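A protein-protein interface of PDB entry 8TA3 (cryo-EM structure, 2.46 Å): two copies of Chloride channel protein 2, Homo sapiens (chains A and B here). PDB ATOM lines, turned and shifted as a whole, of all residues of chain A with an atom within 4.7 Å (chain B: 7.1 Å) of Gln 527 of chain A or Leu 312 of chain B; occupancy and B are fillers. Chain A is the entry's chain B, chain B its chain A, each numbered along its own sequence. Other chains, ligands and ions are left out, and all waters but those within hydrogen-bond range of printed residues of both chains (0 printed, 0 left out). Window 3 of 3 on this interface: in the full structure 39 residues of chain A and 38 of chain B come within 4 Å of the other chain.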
ATOM      1  N   LYS A 307      -4.529 -34.046  11.162  1.00  0.00           N
ATOM      2  CA  LYS A 307      -5.270 -33.915   9.895  1.00  0.00           C
ATOM      3  C   LYS A 307      -6.586 -34.688   9.889  1.00  0.00           C
ATOM      4  O   LYS A 307      -6.583 -35.917   9.943  1.00  0.00           O
ATOM      5  CB  LYS A 307      -4.411 -34.389   8.716  1.00  0.00           C
ATOM      6  CG  LYS A 307      -3.316 -33.387   8.352  1.00  0.00           C
ATOM      7  CD  LYS A 307      -2.366 -33.904   7.266  1.00  0.00           C
ATOM      8  CE  LYS A 307      -3.013 -34.071   5.880  1.00  0.00           C
ATOM      9  NZ  LYS A 307      -3.237 -32.774   5.193  1.00  0.00           N
ATOM     10  N   THR A 308      -7.708 -33.993   9.748  1.00  0.00           N
ATOM     11  CA  THR A 308      -9.022 -34.603   9.507  1.00  0.00           C
ATOM     12  C   THR A 308      -9.288 -34.798   8.013  1.00  0.00           C
ATOM     13  O   THR A 308      -8.676 -34.160   7.158  1.00  0.00           O
ATOM     14  CB  THR A 308     -10.150 -33.817  10.184  1.00  0.00           C
ATOM     15  OG1 THR A 308     -10.202 -32.494   9.734  1.00  0.00           O
ATOM     16  CG2 THR A 308      -9.996 -33.822  11.698  1.00  0.00           C
ATOM     17  N   ARG A 309     -10.193 -35.717   7.686  1.00  0.00           N
ATOM     18  CA  ARG A 309     -10.586 -36.077   6.311  1.00  0.00           C
ATOM     19  C   ARG A 309     -12.106 -36.184   6.210  1.00  0.00           C
ATOM     20  O   ARG A 309     -12.638 -37.227   5.847  1.00  0.00           O
ATOM     21  CB  ARG A 309      -9.879 -37.376   5.883  1.00  0.00           C
ATOM     22  CG  ARG A 309      -8.354 -37.293   5.764  1.00  0.00           C
ATOM     23  CD  ARG A 309      -7.896 -36.420   4.595  1.00  0.00           C
ATOM     24  NE  ARG A 309      -6.430 -36.487   4.457  1.00  0.00           N
ATOM     25  CZ  ARG A 309      -5.713 -36.492   3.349  1.00  0.00           C
ATOM     26  NH1 ARG A 309      -4.426 -36.622   3.429  1.00  0.00           N
ATOM     27  NH2 ARG A 309      -6.235 -36.383   2.166  1.00  0.00           N
ATOM     28  N   PHE A 310     -12.820 -35.136   6.609  1.00  0.00           N
ATOM     29  CA  PHE A 310     -14.277 -35.067   6.465  1.00  0.00           C
ATOM     30  C   PHE A 310     -14.677 -34.629   5.043  1.00  0.00           C
ATOM     31  O   PHE A 310     -13.907 -33.962   4.344  1.00  0.00           O
ATOM     32  CB  PHE A 310     -14.862 -34.146   7.547  1.00  0.00           C
ATOM     33  CG  PHE A 310     -14.403 -34.424   8.973  1.00  0.00           C
ATOM     34  CD1 PHE A 310     -14.188 -35.740   9.432  1.00  0.00           C
ATOM     35  CD2 PHE A 310     -14.177 -33.346   9.847  1.00  0.00           C
ATOM     36  CE1 PHE A 310     -13.706 -35.964  10.733  1.00  0.00           C
ATOM     37  CE2 PHE A 310     -13.719 -33.572  11.153  1.00  0.00           C
ATOM     38  CZ  PHE A 310     -13.466 -34.880  11.590  1.00  0.00           C
ATOM     39  N   PHE A 522      -8.924 -25.187  13.636  1.00  0.00           N
ATOM     40  CA  PHE A 522      -8.817 -25.243  12.172  1.00  0.00           C
ATOM     41  C   PHE A 522      -7.374 -25.432  11.693  1.00  0.00           C
ATOM     42  O   PHE A 522      -7.132 -26.185  10.756  1.00  0.00           O
ATOM     43  CB  PHE A 522      -9.415 -23.987  11.526  1.00  0.00           C
ATOM     44  CG  PHE A 522     -10.800 -23.589  11.988  1.00  0.00           C
ATOM     45  CD1 PHE A 522     -11.791 -24.556  12.239  1.00  0.00           C
ATOM     46  CD2 PHE A 522     -11.101 -22.229  12.181  1.00  0.00           C
ATOM     47  CE1 PHE A 522     -13.042 -24.175  12.745  1.00  0.00           C
ATOM     48  CE2 PHE A 522     -12.352 -21.847  12.691  1.00  0.00           C
ATOM     49  CZ  PHE A 522     -13.312 -22.822  12.999  1.00  0.00           C
ATOM     50  N   THR A 525      -6.244 -29.193  12.607  1.00  0.00           N
ATOM     51  CA  THR A 525      -6.937 -30.214  11.808  1.00  0.00           C
ATOM     52  C   THR A 525      -6.758 -30.046  10.306  1.00  0.00           C
ATOM     53  O   THR A 525      -6.943 -31.004   9.564  1.00  0.00           O
ATOM     54  CB  THR A 525      -8.430 -30.267  12.131  1.00  0.00           C
ATOM     55  OG1 THR A 525      -9.036 -29.021  11.921  1.00  0.00           O
ATOM     56  CG2 THR A 525      -8.703 -30.712  13.563  1.00  0.00           C
ATOM     57  N   GLY A 526      -6.372 -28.857   9.838  1.00  0.00           N
ATOM     58  CA  GLY A 526      -6.189 -28.548   8.426  1.00  0.00           C
ATOM     59  C   GLY A 526      -7.486 -28.429   7.626  1.00  0.00           C
ATOM     60  O   GLY A 526      -7.443 -28.519   6.405  1.00  0.00           O
ATOM     61  N   GLN A 527      -8.637 -28.245   8.279  1.00  0.00           N
ATOM     62  CA  GLN A 527      -9.956 -28.080   7.661  1.00  0.00           C
ATOM     63  C   GLN A 527     -10.784 -27.016   8.394  1.00  0.00           C
ATOM     64  O   GLN A 527     -10.641 -26.823   9.597  1.00  0.00           O
ATOM     65  CB  GLN A 527     -10.727 -29.412   7.627  1.00  0.00           C
ATOM     66  CG  GLN A 527     -10.184 -30.435   6.621  1.00  0.00           C
ATOM     67  CD  GLN A 527     -11.170 -31.575   6.373  1.00  0.00           C
ATOM     68  OE1 GLN A 527     -11.555 -32.315   7.267  1.00  0.00           O
ATOM     69  NE2 GLN A 527     -11.624 -31.768   5.158  1.00  0.00           N
ATOM     70  N   ILE A 528     -11.683 -26.343   7.672  1.00  0.00           N
ATOM     71  CA  ILE A 528     -12.531 -25.248   8.186  1.00  0.00           C
ATOM     72  C   ILE A 528     -14.033 -25.479   7.916  1.00  0.00           C
ATOM     73  O   ILE A 528     -14.848 -24.574   8.028  1.00  0.00           O
ATOM     74  CB  ILE A 528     -11.933 -23.881   7.749  1.00  0.00           C
ATOM     75  CG1 ILE A 528     -12.468 -22.689   8.570  1.00  0.00           C
ATOM     76  CG2 ILE A 528     -12.091 -23.616   6.250  1.00  0.00           C
ATOM     77  CD1 ILE A 528     -11.593 -21.438   8.466  1.00  0.00           C
ATOM     78  N   ALA A 529     -14.435 -26.710   7.592  1.00  0.00           N
ATOM     79  CA  ALA A 529     -15.821 -27.072   7.275  1.00  0.00           C
ATOM     80  C   ALA A 529     -16.806 -27.011   8.466  1.00  0.00           C
ATOM     81  O   ALA A 529     -17.999 -26.810   8.257  1.00  0.00           O
ATOM     82  CB  ALA A 529     -15.811 -28.471   6.658  1.00  0.00           C
ATOM     83  N   PHE B 310      -9.913 -27.686  -4.085  1.00  0.00           N
ATOM     84  CA  PHE B 310      -8.537 -28.174  -4.265  1.00  0.00           C
ATOM     85  C   PHE B 310      -8.266 -29.454  -3.452  1.00  0.00           C
ATOM     86  O   PHE B 310      -8.893 -29.679  -2.416  1.00  0.00           O
ATOM     87  CB  PHE B 310      -7.531 -27.081  -3.879  1.00  0.00           C
ATOM     88  CG  PHE B 310      -7.771 -25.713  -4.490  1.00  0.00           C
ATOM     89  CD1 PHE B 310      -7.913 -25.563  -5.883  1.00  0.00           C
ATOM     90  CD2 PHE B 310      -7.845 -24.582  -3.660  1.00  0.00           C
ATOM     91  CE1 PHE B 310      -8.180 -24.300  -6.433  1.00  0.00           C
ATOM     92  CE2 PHE B 310      -8.084 -23.317  -4.215  1.00  0.00           C
ATOM     93  CZ  PHE B 310      -8.274 -23.179  -5.596  1.00  0.00           C
ATOM     94  N   ARG B 311      -7.311 -30.283  -3.896  1.00  0.00           N
ATOM     95  CA  ARG B 311      -6.857 -31.493  -3.184  1.00  0.00           C
ATOM     96  C   ARG B 311      -6.196 -31.185  -1.833  1.00  0.00           C
ATOM     97  O   ARG B 311      -5.511 -30.174  -1.698  1.00  0.00           O
ATOM     98  CB  ARG B 311      -5.943 -32.332  -4.094  1.00  0.00           C
ATOM     99  CG  ARG B 311      -4.580 -31.699  -4.398  1.00  0.00           C
ATOM    100  CD  ARG B 311      -3.734 -32.618  -5.280  1.00  0.00           C
ATOM    101  NE  ARG B 311      -2.377 -32.068  -5.423  1.00  0.00           N
ATOM    102  CZ  ARG B 311      -1.859 -31.451  -6.465  1.00  0.00           C
ATOM    103  NH1 ARG B 311      -0.721 -30.847  -6.370  1.00  0.00           N
ATOM    104  NH2 ARG B 311      -2.434 -31.409  -7.627  1.00  0.00           N
ATOM    105  N   LEU B 312      -6.355 -32.060  -0.840  1.00  0.00           N
ATOM    106  CA  LEU B 312      -5.674 -31.948   0.463  1.00  0.00           C
ATOM    107  C   LEU B 312      -4.253 -32.547   0.480  1.00  0.00           C
ATOM    108  O   LEU B 312      -3.479 -32.247   1.385  1.00  0.00           O
ATOM    109  CB  LEU B 312      -6.531 -32.604   1.559  1.00  0.00           C
ATOM    110  CG  LEU B 312      -7.862 -31.904   1.880  1.00  0.00           C
ATOM    111  CD1 LEU B 312      -8.629 -32.732   2.907  1.00  0.00           C
ATOM    112  CD2 LEU B 312      -7.678 -30.503   2.466  1.00  0.00           C
ATOM    113  N   ASP B 313      -3.883 -33.373  -0.499  1.00  0.00           N
ATOM    114  CA  ASP B 313      -2.573 -34.037  -0.571  1.00  0.00           C
ATOM    115  C   ASP B 313      -1.606 -33.302  -1.503  1.00  0.00           C
ATOM    116  O   ASP B 313      -1.831 -33.218  -2.707  1.00  0.00           O
ATOM    117  CB  ASP B 313      -2.757 -35.496  -1.015  1.00  0.00           C
ATOM    118  CG  ASP B 313      -3.444 -36.307   0.078  1.00  0.00           C
ATOM    119  OD1 ASP B 313      -2.847 -36.471   1.164  1.00  0.00           O
ATOM    120  OD2 ASP B 313      -4.603 -36.737  -0.097  1.00  0.00           O
ATOM    121  N   PHE B 314      -0.522 -32.767  -0.938  1.00  0.00           N
ATOM    122  CA  PHE B 314       0.517 -31.998  -1.641  1.00  0.00           C
ATOM    123  C   PHE B 314      -0.024 -30.947  -2.637  1.00  0.00           C
ATOM    124  O   PHE B 314       0.335 -30.979  -3.817  1.00  0.00           O
ATOM    125  CB  PHE B 314       1.540 -32.960  -2.263  1.00  0.00           C
ATOM    126  CG  PHE B 314       2.257 -33.807  -1.231  1.00  0.00           C
ATOM    127  CD1 PHE B 314       1.704 -35.028  -0.803  1.00  0.00           C
ATOM    128  CD2 PHE B 314       3.451 -33.344  -0.653  1.00  0.00           C
ATOM    129  CE1 PHE B 314       2.333 -35.776   0.203  1.00  0.00           C
ATOM    130  CE2 PHE B 314       4.090 -34.099   0.344  1.00  0.00           C
ATOM    131  CZ  PHE B 314       3.529 -35.312   0.774  1.00  0.00           C
ATOM    132  N   PRO B 315      -0.883 -29.996  -2.216  1.00  0.00           N
ATOM    133  CA  PRO B 315      -1.439 -28.966  -3.101  1.00  0.00           C
ATOM    134  C   PRO B 315      -0.389 -27.987  -3.658  1.00  0.00           C
ATOM    135  O   PRO B 315      -0.603 -27.413  -4.722  1.00  0.00           O
ATOM    136  CB  PRO B 315      -2.503 -28.244  -2.270  1.00  0.00           C
ATOM    137  CG  PRO B 315      -2.084 -28.481  -0.826  1.00  0.00           C
ATOM    138  CD  PRO B 315      -1.405 -29.842  -0.866  1.00  0.00           C
ATOM    139  N   GLY B 526     -13.645 -21.654   2.068  1.00  0.00           N
ATOM    140  CA  GLY B 526     -13.942 -22.836   2.870  1.00  0.00           C
ATOM    141  C   GLY B 526     -12.819 -23.878   2.904  1.00  0.00           C
ATOM    142  O   GLY B 526     -13.087 -25.043   3.168  1.00  0.00           O
ATOM    143  N   GLN B 527     -11.578 -23.491   2.609  1.00  0.00           N
ATOM    144  CA  GLN B 527     -10.370 -24.314   2.738  1.00  0.00           C
ATOM    145  C   GLN B 527      -9.236 -23.509   3.391  1.00  0.00           C
ATOM    146  O   GLN B 527      -9.189 -22.289   3.289  1.00  0.00           O
ATOM    147  CB  GLN B 527      -9.918 -24.875   1.380  1.00  0.00           C
ATOM    148  CG  GLN B 527     -10.951 -25.799   0.730  1.00  0.00           C
ATOM    149  CD  GLN B 527     -10.400 -26.557  -0.471  1.00  0.00           C
ATOM    150  OE1 GLN B 527     -10.223 -26.014  -1.550  1.00  0.00           O
ATOM    151  NE2 GLN B 527     -10.139 -27.833  -0.340  1.00  0.00           N
ATOM    152  N   ILE B 528      -8.310 -24.204   4.053  1.00  0.00           N
ATOM    153  CA  ILE B 528      -7.160 -23.627   4.768  1.00  0.00           C
ATOM    154  C   ILE B 528      -5.836 -24.313   4.372  1.00  0.00           C
ATOM    155  O   ILE B 528      -4.813 -24.171   5.035  1.00  0.00           O
ATOM    156  CB  ILE B 528      -7.474 -23.548   6.286  1.00  0.00           C
ATOM    157  CG1 ILE B 528      -6.525 -22.598   7.044  1.00  0.00           C
ATOM    158  CG2 ILE B 528      -7.502 -24.929   6.958  1.00  0.00           C
ATOM    159  CD1 ILE B 528      -7.096 -22.106   8.374  1.00  0.00           C
ATOM    160  N   ALA B 529      -5.825 -25.048   3.260  1.00  0.00           N
ATOM    161  CA  ALA B 529      -4.676 -25.807   2.765  1.00  0.00           C
ATOM    162  C   ALA B 529      -3.484 -24.955   2.271  1.00  0.00           C
ATOM    163  O   ALA B 529      -2.358 -25.441   2.259  1.00  0.00           O
ATOM    164  CB  ALA B 529      -5.176 -26.738   1.659  1.00  0.00           C
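NZ of Lys 307 of chain A touches O of Leu 312 of chain B, at 3.9 Å. NH2 of Arg 309 of chain A touches CB of Leu 312 of chain B, 3.8 Å away. Gly 526 of chain A touches Ile 528 of chain B (C to CG2, 3.6 Å). CD1 of Leu 312 of chain B touches NE2 of Gln 527 of chain A, 3.9 Å away. Ile 528 of chain B touches Gln 527 of chain A. Ile 528 of chain A touches Gly 526 of chain B. Ile 528 of chain A touches Gln 527 of chain B (CG2 to N, 3.7 Å).
OD1 of Asp 313 of chain B is in salt-bridge range of NH1 of Arg 309 of chain A.
Gln 527 of chain A touches two residues of chain B. Printed residues of chain B within 4 Å of Lys 307 of chain A: Leu 312. Printed residues of chain A within 4 Å of Ile 528 of chain B: Gly 526 and Gln 527. Printed residues of chain B within 4 Å of Arg 309 of chain A: Leu 312 and Asp 313. Printed residues of chain A within 4 Å of Asp 313 of chain B: Arg 309. Thr 525 of chain A touches none of the printed residues of chain B.
Gly 526 of chain A touches Ile 528 of chain B, and with the chains exchanged Ile 528 of chain A touches Gly 526 of chain B. Gln 527 of chain A touches Ile 528 of chain B, and with the chains exchanged Ile 528 of chain A touches Gln 527 of chain B. Positions printed for both chains: 310, 526, 527, 528 and 529. Of the 8 pairs that touch across the chains among the printed residues, 4 have their exchanged pair printed and touching as well.
O of Phe 310 of chain B is in hydrogen-bond range of NE2 of Gln 527 of chain B (3.0 Å). The guanidinium group (NE) of Arg 311 of chain B is in hydrogen-bond range of the backbone carbonyl oxygen (O) of Asp 313 of chain B, at 3.0 Å. The side-chain amide oxygen (OE1) of Gln 527 of chain A sits at hydrogen-bond distance from the side-chain hydroxyl (OG1) of Thr 308 of chain A, 2.8 Å away. The backbone NH (N) of Phe 310 of chain A lies within hydrogen-bond range of the side-chain amide oxygen (OE1) of Gln 527 of chain A.
Of the 10 printed residues of chain B, 5 touch a printed residue of chain A. Printed residues of chain B that touch a printed residue of chain A: Leu 312, Asp 313, Gly 526, Gln 527 and Ile 528. Hydrophobic or aromatic side chains of chain B within 4 Å of the printed part of chain A: Leu 312 and Ile 528. Along chain B the printed residues that touch a printed residue of chain A span positions 312 to 528. Among the printed residues, Asp or Glu carboxylates within 4 Å of a Lys or Arg side-chain nitrogen of the other chain: Arg 309 of chain A with Asp 313 of chain B.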
